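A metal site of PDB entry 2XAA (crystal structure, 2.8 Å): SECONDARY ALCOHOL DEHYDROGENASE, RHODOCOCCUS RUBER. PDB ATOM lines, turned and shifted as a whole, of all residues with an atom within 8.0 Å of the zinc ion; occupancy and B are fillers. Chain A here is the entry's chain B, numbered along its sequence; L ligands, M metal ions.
N of Ser 40 sits close to SG of Cys 38, at 3.4 Å.
The side-chain hydroxyl (OG1) of Thr 157 sits at hydrogen-bond distance from the side-chain carboxylate (OD1) of Asp 153, at 2.8 Å.
The side-chain carboxylate (OD2) of Asp 41 is in hydrogen-bond range of the backbone NH (N) of Cys 38 (3.5 Å).
ND1 of His 62 sits close to OD1 of Asp 41.
The guanidinium group of Arg 340 lies close to the side-chain sulfur of Cys 38.
Merely in contact with the zinc ion: Ser 40.
Within 4 Å of the zinc ion: Cys 38, Ser 40, His 62 and Asp 153.
Along chain A the residues within 4 Å of the zinc ion span positions 38 to 153.
The zinc ion is bound by OD2 of Asp 153 (2.0 Å), NE2 of His 62 (2.2 Å) and SG of Cys 38 (2.3 Å).
The zinc ion has three donor atoms within binding distance.
The guanidinium group (NH1) of Arg 340 is in salt-bridge range of an oxygen (O8) of the ligand (3.1 Å).
The side-chain hydroxyl of Ser 40 lies within hydrogen-bond range of an oxygen (O13) of the ligand (2.8 Å).
The backbone NH (N) of Ile 271 is in hydrogen-bond range of an oxygen (O12) of the ligand, at 3.1 Å.
The backbone NH of Ser 40 sits close to an oxygen (O13) of the ligand (3.4 Å).
O8 of the ligand sits at hydrogen-bond distance from N of His 39 (3.0 Å).
N of Leu 183 lies within hydrogen-bond range of O9 of the ligand (3.0 Å).
The backbone NH of Trp 295 lies within hydrogen-bond range of an oxygen (O14) of the ligand.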
ATOM      1  N   GLY A  36     -11.787  -2.881  22.432  1.00  0.00           N
ATOM      2  CA  GLY A  36     -11.695  -1.538  21.831  1.00  0.00           C
ATOM      3  C   GLY A  36     -11.818  -1.544  20.315  1.00  0.00           C
ATOM      4  O   GLY A  36     -11.426  -2.509  19.648  1.00  0.00           O
ATOM      5  N   LEU A  37     -12.375  -0.468  19.771  1.00  0.00           N
ATOM      6  CA  LEU A  37     -12.561  -0.324  18.336  1.00  0.00           C
ATOM      7  C   LEU A  37     -11.561   0.653  17.786  1.00  0.00           C
ATOM      8  O   LEU A  37     -11.628   1.844  18.118  1.00  0.00           O
ATOM      9  CB  LEU A  37     -13.930   0.278  18.056  1.00  0.00           C
ATOM     10  CG  LEU A  37     -15.160  -0.608  17.924  1.00  0.00           C
ATOM     11  CD1 LEU A  37     -15.677  -1.045  19.283  1.00  0.00           C
ATOM     12  CD2 LEU A  37     -16.193   0.169  17.138  1.00  0.00           C
ATOM     13  N   CYS A  38     -10.669   0.172  16.935  1.00  0.00           N
ATOM     14  CA  CYS A  38      -9.613   1.026  16.370  1.00  0.00           C
ATOM     15  C   CYS A  38      -9.920   1.415  14.937  1.00  0.00           C
ATOM     16  O   CYS A  38     -10.194   0.533  14.114  1.00  0.00           O
ATOM     17  CB  CYS A  38      -8.254   0.321  16.466  1.00  0.00           C
ATOM     18  SG  CYS A  38      -6.883   1.282  15.830  1.00  0.00           S
ATOM     19  N   HIS A  39      -9.893   2.714  14.637  1.00  0.00           N
ATOM     20  CA  HIS A  39     -10.107   3.165  13.252  1.00  0.00           C
ATOM     21  C   HIS A  39      -9.303   2.341  12.250  1.00  0.00           C
ATOM     22  O   HIS A  39      -9.637   2.285  11.078  1.00  0.00           O
ATOM     23  CB  HIS A  39      -9.794   4.653  13.084  1.00  0.00           C
ATOM     24  CG  HIS A  39     -10.041   5.170  11.697  1.00  0.00           C
ATOM     25  ND1 HIS A  39     -11.206   5.811  11.337  1.00  0.00           N
ATOM     26  CD2 HIS A  39      -9.265   5.123  10.580  1.00  0.00           C
ATOM     27  CE1 HIS A  39     -11.149   6.150  10.063  1.00  0.00           C
ATOM     28  NE2 HIS A  39      -9.985   5.749   9.575  1.00  0.00           N
ATOM     29  N   SER A  40      -8.274   1.663  12.730  1.00  0.00           N
ATOM     30  CA  SER A  40      -7.485   0.814  11.859  1.00  0.00           C
ATOM     31  C   SER A  40      -8.337  -0.273  11.202  1.00  0.00           C
ATOM     32  O   SER A  40      -8.011  -0.744  10.107  1.00  0.00           O
ATOM     33  CB  SER A  40      -6.300   0.180  12.601  1.00  0.00           C
ATOM     34  OG  SER A  40      -5.061   0.662  12.084  1.00  0.00           O
ATOM     35  N   ASP A  41      -9.416  -0.664  11.859  1.00  0.00           N
ATOM     36  CA  ASP A  41     -10.324  -1.651  11.277  1.00  0.00           C
ATOM     37  C   ASP A  41     -11.118  -1.035  10.116  1.00  0.00           C
ATOM     38  O   ASP A  41     -11.235  -1.641   9.043  1.00  0.00           O
ATOM     39  CB  ASP A  41     -11.254  -2.231  12.344  1.00  0.00           C
ATOM     40  CG  ASP A  41     -10.513  -2.717  13.578  1.00  0.00           C
ATOM     41  OD1 ASP A  41      -9.468  -3.375  13.419  1.00  0.00           O
ATOM     42  OD2 ASP A  41     -10.980  -2.456  14.707  1.00  0.00           O
ATOM     43  N   HIS A  62      -8.457  -5.711  17.931  1.00  0.00           N
ATOM     44  CA  HIS A  62      -7.066  -5.822  18.401  1.00  0.00           C
ATOM     45  C   HIS A  62      -6.685  -5.132  19.749  1.00  0.00           C
ATOM     46  O   HIS A  62      -5.501  -5.114  20.150  1.00  0.00           O
ATOM     47  CB  HIS A  62      -6.095  -5.454  17.285  1.00  0.00           C
ATOM     48  CG  HIS A  62      -6.266  -4.054  16.780  1.00  0.00           C
ATOM     49  ND1 HIS A  62      -7.002  -3.758  15.661  1.00  0.00           N
ATOM     50  CD2 HIS A  62      -5.748  -2.875  17.214  1.00  0.00           C
ATOM     51  CE1 HIS A  62      -6.950  -2.451  15.430  1.00  0.00           C
ATOM     52  NE2 HIS A  62      -6.201  -1.901  16.365  1.00  0.00           N
ATOM     53  N   GLU A  63      -7.699  -4.597  20.444  1.00  0.00           N
ATOM     54  CA  GLU A  63      -7.585  -4.060  21.811  1.00  0.00           C
ATOM     55  C   GLU A  63      -8.392  -4.923  22.814  1.00  0.00           C
ATOM     56  O   GLU A  63      -9.587  -4.727  22.976  1.00  0.00           O
ATOM     57  CB  GLU A  63      -8.096  -2.603  21.897  1.00  0.00           C
ATOM     58  CG  GLU A  63      -7.427  -1.560  21.018  1.00  0.00           C
ATOM     59  CD  GLU A  63      -7.995  -0.155  21.289  1.00  0.00           C
ATOM     60  OE1 GLU A  63      -9.063  -0.076  21.929  1.00  0.00           O
ATOM     61  OE2 GLU A  63      -7.398   0.876  20.865  1.00  0.00           O
ATOM     62  N   LEU A 119      -6.221  -9.336  13.634  1.00  0.00           N
ATOM     63  CA  LEU A 119      -5.464  -8.868  12.479  1.00  0.00           C
ATOM     64  C   LEU A 119      -4.810  -9.994  11.663  1.00  0.00           C
ATOM     65  O   LEU A 119      -3.694  -9.845  11.148  1.00  0.00           O
ATOM     66  CB  LEU A 119      -4.417  -7.834  12.922  1.00  0.00           C
ATOM     67  CG  LEU A 119      -4.887  -6.404  13.220  1.00  0.00           C
ATOM     68  CD1 LEU A 119      -3.758  -5.474  13.742  1.00  0.00           C
ATOM     69  CD2 LEU A 119      -5.557  -5.807  11.947  1.00  0.00           C
ATOM     70  N   THR A 152      -4.293  -0.739  25.235  1.00  0.00           N
ATOM     71  CA  THR A 152      -3.469  -1.708  24.466  1.00  0.00           C
ATOM     72  C   THR A 152      -3.060  -1.186  23.098  1.00  0.00           C
ATOM     73  O   THR A 152      -2.152  -1.749  22.483  1.00  0.00           O
ATOM     74  CB  THR A 152      -4.116  -3.140  24.325  1.00  0.00           C
ATOM     75  OG1 THR A 152      -5.222  -3.078  23.406  1.00  0.00           O
ATOM     76  CG2 THR A 152      -4.579  -3.721  25.679  1.00  0.00           C
ATOM     77  N   ASP A 153      -3.708  -0.139  22.617  1.00  0.00           N
ATOM     78  CA  ASP A 153      -3.402   0.370  21.302  1.00  0.00           C
ATOM     79  C   ASP A 153      -3.465   1.891  21.275  1.00  0.00           C
ATOM     80  O   ASP A 153      -2.446   2.541  21.000  1.00  0.00           O
ATOM     81  CB  ASP A 153      -4.344  -0.270  20.276  1.00  0.00           C
ATOM     82  CG  ASP A 153      -3.999   0.086  18.828  1.00  0.00           C
ATOM     83  OD1 ASP A 153      -2.921   0.700  18.589  1.00  0.00           O
ATOM     84  OD2 ASP A 153      -4.835  -0.236  17.940  1.00  0.00           O
ATOM     85  N   ALA A 154      -4.645   2.464  21.553  1.00  0.00           N
ATOM     86  CA  ALA A 154      -4.791   3.923  21.626  1.00  0.00           C
ATOM     87  C   ALA A 154      -3.894   4.504  22.691  1.00  0.00           C
ATOM     88  O   ALA A 154      -3.586   5.699  22.643  1.00  0.00           O
ATOM     89  CB  ALA A 154      -6.232   4.332  21.884  1.00  0.00           C
ATOM     90  N   THR A 157       0.296   2.869  21.202  1.00  0.00           N
ATOM     91  CA  THR A 157       0.804   3.408  19.963  1.00  0.00           C
ATOM     92  C   THR A 157       1.354   4.809  20.179  1.00  0.00           C
ATOM     93  O   THR A 157       2.518   5.039  19.822  1.00  0.00           O
ATOM     94  CB  THR A 157      -0.201   3.337  18.834  1.00  0.00           C
ATOM     95  OG1 THR A 157      -0.472   1.956  18.544  1.00  0.00           O
ATOM     96  CG2 THR A 157       0.324   4.017  17.568  1.00  0.00           C
ATOM     97  N   LEU A 183      -6.432   7.625  19.527  1.00  0.00           N
ATOM     98  CA  LEU A 183      -5.017   7.626  19.888  1.00  0.00           C
ATOM     99  C   LEU A 183      -4.564   8.998  20.387  1.00  0.00           C
ATOM    100  O   LEU A 183      -3.824   9.090  21.390  1.00  0.00           O
ATOM    101  CB  LEU A 183      -4.161   7.207  18.692  1.00  0.00           C
ATOM    102  CG  LEU A 183      -4.019   5.719  18.389  1.00  0.00           C
ATOM    103  CD1 LEU A 183      -5.319   5.076  17.973  1.00  0.00           C
ATOM    104  CD2 LEU A 183      -3.015   5.571  17.294  1.00  0.00           C
ATOM    105  N   ILE A 271      -2.746   6.378   9.216  1.00  0.00           N
ATOM    106  CA  ILE A 271      -2.639   5.714   7.917  1.00  0.00           C
ATOM    107  C   ILE A 271      -3.592   6.301   6.875  1.00  0.00           C
ATOM    108  O   ILE A 271      -4.799   6.107   6.935  1.00  0.00           O
ATOM    109  CB  ILE A 271      -2.868   4.171   8.017  1.00  0.00           C
ATOM    110  CG1 ILE A 271      -2.507   3.675   9.438  1.00  0.00           C
ATOM    111  CG2 ILE A 271      -2.110   3.433   6.885  1.00  0.00           C
ATOM    112  CD1 ILE A 271      -2.224   2.144   9.595  1.00  0.00           C
ATOM    113  N   TYR A 294       5.085   1.678  14.543  1.00  0.00           N
ATOM    114  CA  TYR A 294       4.065   0.668  14.538  1.00  0.00           C
ATOM    115  C   TYR A 294       3.845   0.196  15.948  1.00  0.00           C
ATOM    116  O   TYR A 294       4.754  -0.390  16.565  1.00  0.00           O
ATOM    117  CB  TYR A 294       4.487  -0.522  13.649  1.00  0.00           C
ATOM    118  CG  TYR A 294       3.625  -1.761  13.797  1.00  0.00           C
ATOM    119  CD1 TYR A 294       2.315  -1.811  13.260  1.00  0.00           C
ATOM    120  CD2 TYR A 294       4.119  -2.872  14.486  1.00  0.00           C
ATOM    121  CE1 TYR A 294       1.513  -2.977  13.419  1.00  0.00           C
ATOM    122  CE2 TYR A 294       3.341  -4.047  14.646  1.00  0.00           C
ATOM    123  CZ  TYR A 294       2.055  -4.075  14.110  1.00  0.00           C
ATOM    124  OH  TYR A 294       1.332  -5.229  14.275  1.00  0.00           O
ATOM    125  N   TRP A 295       2.646   0.437  16.449  1.00  0.00           N
ATOM    126  CA  TRP A 295       2.206  -0.116  17.701  1.00  0.00           C
ATOM    127  C   TRP A 295       3.250   0.136  18.806  1.00  0.00           C
ATOM    128  O   TRP A 295       3.703   1.259  18.905  1.00  0.00           O
ATOM    129  CB  TRP A 295       1.900  -1.582  17.520  1.00  0.00           C
ATOM    130  CG  TRP A 295       0.751  -1.982  18.294  1.00  0.00           C
ATOM    131  CD1 TRP A 295       0.302  -1.401  19.434  1.00  0.00           C
ATOM    132  CD2 TRP A 295      -0.127  -3.056  18.009  1.00  0.00           C
ATOM    133  NE1 TRP A 295      -0.820  -2.049  19.884  1.00  0.00           N
ATOM    134  CE2 TRP A 295      -1.109  -3.065  19.027  1.00  0.00           C
ATOM    135  CE3 TRP A 295      -0.183  -4.020  17.008  1.00  0.00           C
ATOM    136  CZ2 TRP A 295      -2.123  -4.014  19.061  1.00  0.00           C
ATOM    137  CZ3 TRP A 295      -1.204  -4.965  17.048  1.00  0.00           C
ATOM    138  CH2 TRP A 295      -2.156  -4.950  18.053  1.00  0.00           C
ATOM    139  N   ARG A 340     -13.018   6.665  22.355  1.00  0.00           N
ATOM    140  CA  ARG A 340     -13.015   5.287  21.883  1.00  0.00           C
ATOM    141  C   ARG A 340     -14.363   4.643  22.103  1.00  0.00           C
ATOM    142  O   ARG A 340     -14.984   4.838  23.140  1.00  0.00           O
ATOM    143  CB  ARG A 340     -11.943   4.456  22.597  1.00  0.00           C
ATOM    144  CG  ARG A 340     -10.676   4.275  21.767  1.00  0.00           C
ATOM    145  CD  ARG A 340     -10.743   2.971  21.009  1.00  0.00           C
ATOM    146  NE  ARG A 340      -9.494   2.662  20.326  1.00  0.00           N
ATOM    147  CZ  ARG A 340      -9.056   3.293  19.240  1.00  0.00           C
ATOM    148  NH1 ARG A 340      -9.750   4.302  18.722  1.00  0.00           N
ATOM    149  NH2 ARG A 340      -7.930   2.912  18.684  1.00  0.00           N
HETATM  150  P1  LIG L   1     -10.245   8.158  15.330  1.00  0.00           P
HETATM  151  O1  LIG L   1     -11.355   8.102  14.361  1.00  0.00           O
HETATM  152  O2  LIG L   1     -10.628   7.550  16.628  1.00  0.00           O
HETATM  153  O3  LIG L   1      -9.844   9.709  15.429  1.00  0.00           O
HETATM  154  C1  LIG L   1      -9.699  10.518  14.283  1.00  0.00           C
HETATM  155  C2  LIG L   1      -9.601  11.990  14.694  1.00  0.00           C
HETATM  156  O4  LIG L   1      -8.856  12.678  13.697  1.00  0.00           O
HETATM  157  C3  LIG L   1     -10.968  12.657  14.785  1.00  0.00           C
HETATM  158  O5  LIG L   1     -11.112  13.567  15.864  1.00  0.00           O
HETATM  159  C4  LIG L   1     -11.043  13.412  13.463  1.00  0.00           C
HETATM  160  O6  LIG L   1     -11.915  14.516  13.492  1.00  0.00           O
HETATM  161  C5  LIG L   1      -9.588  13.812  13.259  1.00  0.00           C
HETATM  162  N1  LIG L   1      -9.259  14.204  11.875  1.00  0.00           N
HETATM  163  C6  LIG L   1      -9.675  13.655  10.674  1.00  0.00           C
HETATM  164  N2  LIG L   1      -9.091  14.338   9.642  1.00  0.00           N
HETATM  165  C7  LIG L   1      -8.316  15.326  10.188  1.00  0.00           C
HETATM  166  C8  LIG L   1      -7.488  16.309   9.654  1.00  0.00           C
HETATM  167  N3  LIG L   1      -7.594  16.639   8.382  1.00  0.00           N
HETATM  168  N4  LIG L   1      -6.803  17.177  10.466  1.00  0.00           N
HETATM  169  C9  LIG L   1      -6.926  17.081  11.824  1.00  0.00           C
HETATM  170  N5  LIG L   1      -7.717  16.103  12.367  1.00  0.00           N
HETATM  171  C10 LIG L   1      -8.410  15.243  11.577  1.00  0.00           C
HETATM  172  O7  LIG L   1      -8.966   7.414  14.714  1.00  0.00           O
HETATM  173  P2  LIG L   1      -8.096   6.483  15.671  1.00  0.00           P
HETATM  174  O8  LIG L   1      -8.813   5.201  15.924  1.00  0.00           O
HETATM  175  O9  LIG L   1      -7.694   7.307  16.834  1.00  0.00           O
HETATM  176  O10 LIG L   1      -6.776   6.250  14.767  1.00  0.00           O
HETATM  177  C11 LIG L   1      -6.069   7.322  14.165  1.00  0.00           C
HETATM  178  C12 LIG L   1      -5.141   6.811  13.047  1.00  0.00           C
HETATM  179  O11 LIG L   1      -3.986   6.136  13.569  1.00  0.00           O
HETATM  180  C13 LIG L   1      -5.833   5.832  12.083  1.00  0.00           C
HETATM  181  O12 LIG L   1      -5.419   6.130  10.758  1.00  0.00           O
HETATM  182  C14 LIG L   1      -5.345   4.490  12.635  1.00  0.00           C
HETATM  183  O13 LIG L   1      -5.464   3.370  11.796  1.00  0.00           O
HETATM  184  C15 LIG L   1      -3.915   4.851  12.974  1.00  0.00           C
HETATM  185  N6  LIG L   1      -3.262   3.898  13.865  1.00  0.00           N
HETATM  186  C16 LIG L   1      -1.951   3.611  13.596  1.00  0.00           C
HETATM  187  C17 LIG L   1      -1.262   2.711  14.403  1.00  0.00           C
HETATM  188  C18 LIG L   1       0.214   2.495  14.202  1.00  0.00           C
HETATM  189  O14 LIG L   1       0.767   1.257  14.616  1.00  0.00           O
HETATM  190  N7  LIG L   1       0.942   3.445  13.608  1.00  0.00           N
HETATM  191  C19 LIG L   1      -1.921   2.104  15.480  1.00  0.00           C
HETATM  192  C20 LIG L   1      -3.251   2.409  15.728  1.00  0.00           C
HETATM  193  C21 LIG L   1      -3.926   3.307  14.903  1.00  0.00           C
HETATM  194 ZN    ZN M   1      -5.075  -0.095  15.956  1.00  0.00          ZN
